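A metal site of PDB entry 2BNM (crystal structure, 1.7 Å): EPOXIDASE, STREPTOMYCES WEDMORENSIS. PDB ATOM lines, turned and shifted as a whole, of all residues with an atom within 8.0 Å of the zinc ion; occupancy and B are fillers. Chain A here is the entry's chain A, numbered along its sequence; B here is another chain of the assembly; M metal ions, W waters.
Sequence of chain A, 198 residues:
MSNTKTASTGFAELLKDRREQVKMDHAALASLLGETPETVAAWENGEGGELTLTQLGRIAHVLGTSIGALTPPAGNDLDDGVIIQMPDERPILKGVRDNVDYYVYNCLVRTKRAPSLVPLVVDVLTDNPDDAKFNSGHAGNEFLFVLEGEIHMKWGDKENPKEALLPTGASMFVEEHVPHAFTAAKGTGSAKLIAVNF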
ATOM      1  N   ASN A  99     -10.040  11.026  -8.085  1.00  0.00           N
ATOM      2  CA  ASN A  99      -9.604  11.930  -7.014  1.00  0.00           C
ATOM      3  C   ASN A  99      -8.477  11.346  -6.194  1.00  0.00           C
ATOM      4  O   ASN A  99      -8.673  10.923  -5.040  1.00  0.00           O
ATOM      5  CB  ASN A  99     -10.788  12.316  -6.140  1.00  0.00           C
ATOM      6  CG  ASN A  99     -11.809  13.161  -6.871  1.00  0.00           C
ATOM      7  OD1 ASN A  99     -11.465  13.870  -7.836  1.00  0.00           O
ATOM      8  ND2 ASN A  99     -13.051  13.113  -6.428  1.00  0.00           N
ATOM      9  N   LEU A 120     -14.222  12.334   6.673  1.00  0.00           N
ATOM     10  CA  LEU A 120     -12.866  12.487   6.133  1.00  0.00           C
ATOM     11  C   LEU A 120     -12.428  13.924   6.316  1.00  0.00           C
ATOM     12  O   LEU A 120     -13.254  14.836   6.202  1.00  0.00           O
ATOM     13  CB  LEU A 120     -12.888  12.225   4.638  1.00  0.00           C
ATOM     14  CG  LEU A 120     -13.495  10.929   4.116  1.00  0.00           C
ATOM     15  CD1 LEU A 120     -13.766  11.015   2.644  1.00  0.00           C
ATOM     16  CD2 LEU A 120     -12.575   9.786   4.446  1.00  0.00           C
ATOM     17  N   VAL A 122     -10.394  16.122   3.941  1.00  0.00           N
ATOM     18  CA  VAL A 122      -9.938  16.054   2.561  1.00  0.00           C
ATOM     19  C   VAL A 122      -9.003  17.238   2.344  1.00  0.00           C
ATOM     20  O   VAL A 122      -9.402  18.398   2.453  1.00  0.00           O
ATOM     21  CB  VAL A 122     -11.074  16.082   1.548  1.00  0.00           C
ATOM     22  CG1 VAL A 122     -10.489  15.898   0.141  1.00  0.00           C
ATOM     23  CG2 VAL A 122     -12.098  14.957   1.828  1.00  0.00           C
ATOM     24  N   ASN A 135     -17.809  13.561  -9.910  1.00  0.00           N
ATOM     25  CA  ASN A 135     -18.227  12.195  -9.640  1.00  0.00           C
ATOM     26  C   ASN A 135     -19.629  11.947 -10.204  1.00  0.00           C
ATOM     27  O   ASN A 135     -20.163  12.759 -10.981  1.00  0.00           O
ATOM     28  CB  ASN A 135     -18.102  11.828  -8.159  1.00  0.00           C
ATOM     29  CG  ASN A 135     -19.005  12.674  -7.278  1.00  0.00           C
ATOM     30  OD1 ASN A 135     -20.044  13.158  -7.727  1.00  0.00           O
ATOM     31  ND2 ASN A 135     -18.626  12.848  -6.025  1.00  0.00           N
ATOM     32  N   GLY A 137     -22.124  11.103  -8.101  1.00  0.00           N
ATOM     33  CA  GLY A 137     -22.937  11.177  -6.906  1.00  0.00           C
ATOM     34  C   GLY A 137     -22.574  10.075  -5.934  1.00  0.00           C
ATOM     35  O   GLY A 137     -22.040   9.021  -6.341  1.00  0.00           O
ATOM     36  N   HIS A 138     -22.838  10.313  -4.660  1.00  0.00           N
ATOM     37  CA  HIS A 138     -22.603   9.330  -3.616  1.00  0.00           C
ATOM     38  C   HIS A 138     -23.860   8.486  -3.376  1.00  0.00           C
ATOM     39  O   HIS A 138     -24.978   8.930  -3.630  1.00  0.00           O
ATOM     40  CB  HIS A 138     -22.217   9.991  -2.285  1.00  0.00           C
ATOM     41  CG  HIS A 138     -21.011  10.889  -2.339  1.00  0.00           C
ATOM     42  ND1 HIS A 138     -19.801  10.499  -2.880  1.00  0.00           N
ATOM     43  CD2 HIS A 138     -20.826  12.147  -1.878  1.00  0.00           C
ATOM     44  CE1 HIS A 138     -18.932  11.478  -2.775  1.00  0.00           C
ATOM     45  NE2 HIS A 138     -19.513  12.498  -2.154  1.00  0.00           N
ATOM     46  N   GLY A 140     -25.072   7.834  -0.426  1.00  0.00           N
ATOM     47  CA  GLY A 140     -25.802   8.413   0.709  1.00  0.00           C
ATOM     48  C   GLY A 140     -25.607   9.932   0.739  1.00  0.00           C
ATOM     49  O   GLY A 140     -24.958  10.470  -0.153  1.00  0.00           O
ATOM     50  N   ASN A 141     -26.172  10.592   1.746  1.00  0.00           N
ATOM     51  CA  ASN A 141     -26.079  12.052   1.890  1.00  0.00           C
ATOM     52  C   ASN A 141     -24.711  12.442   2.409  1.00  0.00           C
ATOM     53  O   ASN A 141     -23.983  11.605   2.955  1.00  0.00           O
ATOM     54  CB  ASN A 141     -27.144  12.545   2.852  1.00  0.00           C
ATOM     55  CG  ASN A 141     -28.578  12.408   2.307  1.00  0.00           C
ATOM     56  OD1 ASN A 141     -28.832  12.470   1.085  1.00  0.00           O
ATOM     57  ND2 ASN A 141     -29.531  12.266   3.229  1.00  0.00           N
ATOM     58  N   GLU A 142     -24.348  13.729   2.237  1.00  0.00           N
ATOM     59  CA  GLU A 142     -23.030  14.210   2.671  1.00  0.00           C
ATOM     60  C   GLU A 142     -23.155  15.600   3.275  1.00  0.00           C
ATOM     61  O   GLU A 142     -23.845  16.457   2.730  1.00  0.00           O
ATOM     62  CB  GLU A 142     -22.063  14.219   1.483  1.00  0.00           C
ATOM     63  CG  GLU A 142     -20.620  14.486   1.872  1.00  0.00           C
ATOM     64  CD  GLU A 142     -19.704  14.437   0.648  1.00  0.00           C
ATOM     65  OE1 GLU A 142     -18.629  13.802   0.721  1.00  0.00           O
ATOM     66  OE2 GLU A 142     -20.056  15.025  -0.374  1.00  0.00           O
ATOM     67  N   PHE A 143     -22.502  15.802   4.413  1.00  0.00           N
ATOM     68  CA  PHE A 143     -22.413  17.097   5.017  1.00  0.00           C
ATOM     69  C   PHE A 143     -20.953  17.508   4.903  1.00  0.00           C
ATOM     70  O   PHE A 143     -20.071  16.697   5.191  1.00  0.00           O
ATOM     71  CB  PHE A 143     -22.753  16.995   6.493  1.00  0.00           C
ATOM     72  CG  PHE A 143     -22.268  18.176   7.296  1.00  0.00           C
ATOM     73  CD1 PHE A 143     -22.967  19.388   7.261  1.00  0.00           C
ATOM     74  CD2 PHE A 143     -21.075  18.104   8.040  1.00  0.00           C
ATOM     75  CE1 PHE A 143     -22.505  20.516   7.992  1.00  0.00           C
ATOM     76  CE2 PHE A 143     -20.609  19.215   8.752  1.00  0.00           C
ATOM     77  CZ  PHE A 143     -21.338  20.419   8.708  1.00  0.00           C
ATOM     78  N   LEU A 144     -20.712  18.775   4.537  1.00  0.00           N
ATOM     79  CA  LEU A 144     -19.346  19.290   4.450  1.00  0.00           C
ATOM     80  C   LEU A 144     -19.131  20.613   5.185  1.00  0.00           C
ATOM     81  O   LEU A 144     -20.058  21.399   5.355  1.00  0.00           O
ATOM     82  CB  LEU A 144     -18.940  19.437   2.980  1.00  0.00           C
ATOM     83  CG  LEU A 144     -19.061  18.208   2.081  1.00  0.00           C
ATOM     84  CD1 LEU A 144     -20.387  18.250   1.327  1.00  0.00           C
ATOM     85  CD2 LEU A 144     -17.855  18.113   1.104  1.00  0.00           C
ATOM     86  N   MET A 172     -22.232  22.799   3.863  1.00  0.00           N
ATOM     87  CA  MET A 172     -22.966  22.374   2.691  1.00  0.00           C
ATOM     88  C   MET A 172     -23.564  21.002   2.958  1.00  0.00           C
ATOM     89  O   MET A 172     -23.003  20.190   3.729  1.00  0.00           O
ATOM     90  CB  MET A 172     -22.057  22.319   1.465  1.00  0.00           C
ATOM     91  CG  MET A 172     -22.696  21.738   0.201  1.00  0.00           C
ATOM     92  SD  MET A 172     -21.474  22.041  -1.075  1.00  0.00           S
ATOM     93  CE  MET A 172     -21.955  21.004  -2.456  1.00  0.00           C
ATOM     94  N   VAL A 174     -25.112  17.837   0.543  1.00  0.00           N
ATOM     95  CA  VAL A 174     -25.254  17.302  -0.835  1.00  0.00           C
ATOM     96  C   VAL A 174     -26.083  16.033  -0.737  1.00  0.00           C
ATOM     97  O   VAL A 174     -25.681  15.072  -0.074  1.00  0.00           O
ATOM     98  CB  VAL A 174     -23.890  16.964  -1.523  1.00  0.00           C
ATOM     99  CG1 VAL A 174     -24.130  16.545  -2.978  1.00  0.00           C
ATOM    100  CG2 VAL A 174     -22.951  18.155  -1.487  1.00  0.00           C
ATOM    101  N   GLU A 175     -27.250  16.037  -1.371  1.00  0.00           N
ATOM    102  CA  GLU A 175     -28.108  14.840  -1.314  1.00  0.00           C
ATOM    103  C   GLU A 175     -27.499  13.662  -2.082  1.00  0.00           C
ATOM    104  O   GLU A 175     -26.755  13.858  -3.054  1.00  0.00           O
ATOM    105  CB  GLU A 175     -29.451  15.158  -1.952  1.00  0.00           C
ATOM    106  CG  GLU A 175     -30.577  14.268  -1.471  1.00  0.00           C
ATOM    107  CD  GLU A 175     -31.922  14.789  -1.948  1.00  0.00           C
ATOM    108  OE1 GLU A 175     -31.974  15.336  -3.051  1.00  0.00           O
ATOM    109  OE2 GLU A 175     -32.891  14.698  -1.188  1.00  0.00           O
ATOM    110  N   VAL A 178     -26.252  13.155  -6.182  1.00  0.00           N
ATOM    111  CA  VAL A 178     -25.984  14.408  -6.866  1.00  0.00           C
ATOM    112  C   VAL A 178     -24.516  14.476  -7.254  1.00  0.00           C
ATOM    113  O   VAL A 178     -23.657  14.490  -6.382  1.00  0.00           O
ATOM    114  CB  VAL A 178     -26.303  15.624  -5.971  1.00  0.00           C
ATOM    115  CG1 VAL A 178     -25.933  16.945  -6.656  1.00  0.00           C
ATOM    116  CG2 VAL A 178     -27.793  15.575  -5.550  1.00  0.00           C
ATOM    117  N   PRO A 179     -24.215  14.571  -8.550  1.00  0.00           N
ATOM    118  CA  PRO A 179     -22.811  14.646  -8.978  1.00  0.00           C
ATOM    119  C   PRO A 179     -22.220  15.954  -8.502  1.00  0.00           C
ATOM    120  O   PRO A 179     -22.894  16.991  -8.504  1.00  0.00           O
ATOM    121  CB  PRO A 179     -22.893  14.646 -10.508  1.00  0.00           C
ATOM    122  CG  PRO A 179     -24.262  14.188 -10.835  1.00  0.00           C
ATOM    123  CD  PRO A 179     -25.132  14.603  -9.699  1.00  0.00           C
ATOM    124  N   HIS A 180     -20.953  15.911  -8.100  1.00  0.00           N
ATOM    125  CA  HIS A 180     -20.295  17.153  -7.685  1.00  0.00           C
ATOM    126  C   HIS A 180     -18.780  17.036  -7.730  1.00  0.00           C
ATOM    127  O   HIS A 180     -18.222  15.939  -7.918  1.00  0.00           O
ATOM    128  CB  HIS A 180     -20.753  17.574  -6.270  1.00  0.00           C
ATOM    129  CG  HIS A 180     -20.586  16.503  -5.238  1.00  0.00           C
ATOM    130  ND1 HIS A 180     -21.375  15.369  -5.201  1.00  0.00           N
ATOM    131  CD2 HIS A 180     -19.691  16.371  -4.236  1.00  0.00           C
ATOM    132  CE1 HIS A 180     -20.999  14.602  -4.192  1.00  0.00           C
ATOM    133  NE2 HIS A 180     -19.987  15.191  -3.594  1.00  0.00           N
ATOM    134  N   ALA A 181     -18.124  18.170  -7.545  1.00  0.00           N
ATOM    135  CA  ALA A 181     -16.649  18.262  -7.551  1.00  0.00           C
ATOM    136  C   ALA A 181     -16.214  19.492  -6.784  1.00  0.00           C
ATOM    137  O   ALA A 181     -16.941  20.493  -6.682  1.00  0.00           O
ATOM    138  CB  ALA A 181     -16.138  18.329  -8.995  1.00  0.00           C
ATOM    139  N   PHE A 182     -15.008  19.424  -6.206  1.00  0.00           N
ATOM    140  CA  PHE A 182     -14.453  20.594  -5.528  1.00  0.00           C
ATOM    141  C   PHE A 182     -12.997  20.761  -5.873  1.00  0.00           C
ATOM    142  O   PHE A 182     -12.276  19.775  -6.012  1.00  0.00           O
ATOM    143  CB  PHE A 182     -14.369  20.326  -3.999  1.00  0.00           C
ATOM    144  CG  PHE A 182     -15.654  19.973  -3.334  1.00  0.00           C
ATOM    145  CD1 PHE A 182     -15.959  18.640  -3.038  1.00  0.00           C
ATOM    146  CD2 PHE A 182     -16.544  20.966  -2.943  1.00  0.00           C
ATOM    147  CE1 PHE A 182     -17.149  18.288  -2.401  1.00  0.00           C
ATOM    148  CE2 PHE A 182     -17.753  20.634  -2.294  1.00  0.00           C
ATOM    149  CZ  PHE A 182     -18.049  19.282  -2.029  1.00  0.00           C
ATOM    150  N   LEU A 193     -11.316  20.414   3.556  1.00  0.00           N
ATOM    151  CA  LEU A 193     -12.713  20.278   3.946  1.00  0.00           C
ATOM    152  C   LEU A 193     -12.854  19.088   4.885  1.00  0.00           C
ATOM    153  O   LEU A 193     -12.018  18.179   4.856  1.00  0.00           O
ATOM    154  CB  LEU A 193     -13.476  19.759   2.708  1.00  0.00           C
ATOM    155  CG  LEU A 193     -13.866  20.474   1.428  1.00  0.00           C
ATOM    156  CD1 LEU A 193     -14.140  19.469   0.385  1.00  0.00           C
ATOM    157  CD2 LEU A 193     -15.116  21.273   1.639  1.00  0.00           C
ATOM    158  N   ALA A 195     -15.522  16.160   5.178  1.00  0.00           N
ATOM    159  CA  ALA A 195     -16.620  15.617   4.384  1.00  0.00           C
ATOM    160  C   ALA A 195     -17.184  14.466   5.206  1.00  0.00           C
ATOM    161  O   ALA A 195     -16.447  13.559   5.579  1.00  0.00           O
ATOM    162  CB  ALA A 195     -16.138  15.102   3.068  1.00  0.00           C
ATOM    163  N   VAL A 196     -18.456  14.549   5.555  1.00  0.00           N
ATOM    164  CA  VAL A 196     -19.074  13.505   6.387  1.00  0.00           C
ATOM    165  C   VAL A 196     -20.155  12.806   5.581  1.00  0.00           C
ATOM    166  O   VAL A 196     -21.247  13.339   5.424  1.00  0.00           O
ATOM    167  CB  VAL A 196     -19.703  14.088   7.681  1.00  0.00           C
ATOM    168  CG1 VAL A 196     -20.253  12.967   8.578  1.00  0.00           C
ATOM    169  CG2 VAL A 196     -18.680  14.936   8.471  1.00  0.00           C
ATOM    170  N   ASN A 197     -19.835  11.647   5.004  1.00  0.00           N
ATOM    171  CA  ASN A 197     -20.848  10.815   4.383  1.00  0.00           C
ATOM    172  C   ASN A 197     -21.594  10.088   5.467  1.00  0.00           C
ATOM    173  O   ASN A 197     -20.985   9.648   6.426  1.00  0.00           O
ATOM    174  CB  ASN A 197     -20.264   9.821   3.389  1.00  0.00           C
ATOM    175  CG  ASN A 197     -20.530  10.236   1.952  1.00  0.00           C
ATOM    176  OD1 ASN A 197     -21.639  10.019   1.381  1.00  0.00           O
ATOM    177  ND2 ASN A 197     -19.542  10.891   1.365  1.00  0.00           N
ATOM    178  N   LYS B  23     -12.385   4.637   0.711  1.00  0.00           N
ATOM    179  CA  LYS B  23     -11.237   5.257   0.059  1.00  0.00           C
ATOM    180  C   LYS B  23      -9.996   4.351  -0.031  1.00  0.00           C
ATOM    181  O   LYS B  23      -8.873   4.854  -0.188  1.00  0.00           O
ATOM    182  CB  LYS B  23     -10.901   6.594   0.712  1.00  0.00           C
ATOM    183  CG  LYS B  23     -12.089   7.546   0.734  1.00  0.00           C
ATOM    184  CD  LYS B  23     -12.493   7.841  -0.694  1.00  0.00           C
ATOM    185  CE  LYS B  23     -13.410   8.985  -0.817  1.00  0.00           C
ATOM    186  NZ  LYS B  23     -13.341   9.366  -2.262  1.00  0.00           N
HETATM  187 ZN    ZN M   1     -18.983  14.366  -1.942  1.00  0.00          ZN
HETATM  188  O   HOH W   1     -16.277  13.928  -4.073  1.00  0.00           O
HETATM  189  O   HOH W   2     -17.090  14.915  -1.945  1.00  0.00           O
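OE1 of Glu 142 lies within hydrogen-bond range of ND2 of Asn 197.
The backbone NH of Val 174 sits at hydrogen-bond distance from the backbone carbonyl oxygen of Glu 142 (2.9 Å).
The backbone NH of His 180 lies within hydrogen-bond range of the side-chain amide oxygen of Asn 135, at 2.9 Å.
A ring nitrogen (ND1) of His 180 lies within hydrogen-bond range of the backbone carbonyl oxygen (O) of Val 178 (2.7 Å).
The nearest printed residue that does not touch the zinc ion is Phe 182 (4.4 Å).
The zinc ion is bound by a ring nitrogen (NE2) of His 138 (2.0 Å), water W2 (2.0 Å), the side-chain carboxylate of Glu 142 (2.0 Å) and a ring nitrogen (NE2) of His 180 (2.1 Å).
Slightly farther from the zinc ion lies OE1 of Glu 142 (2.7 Å).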
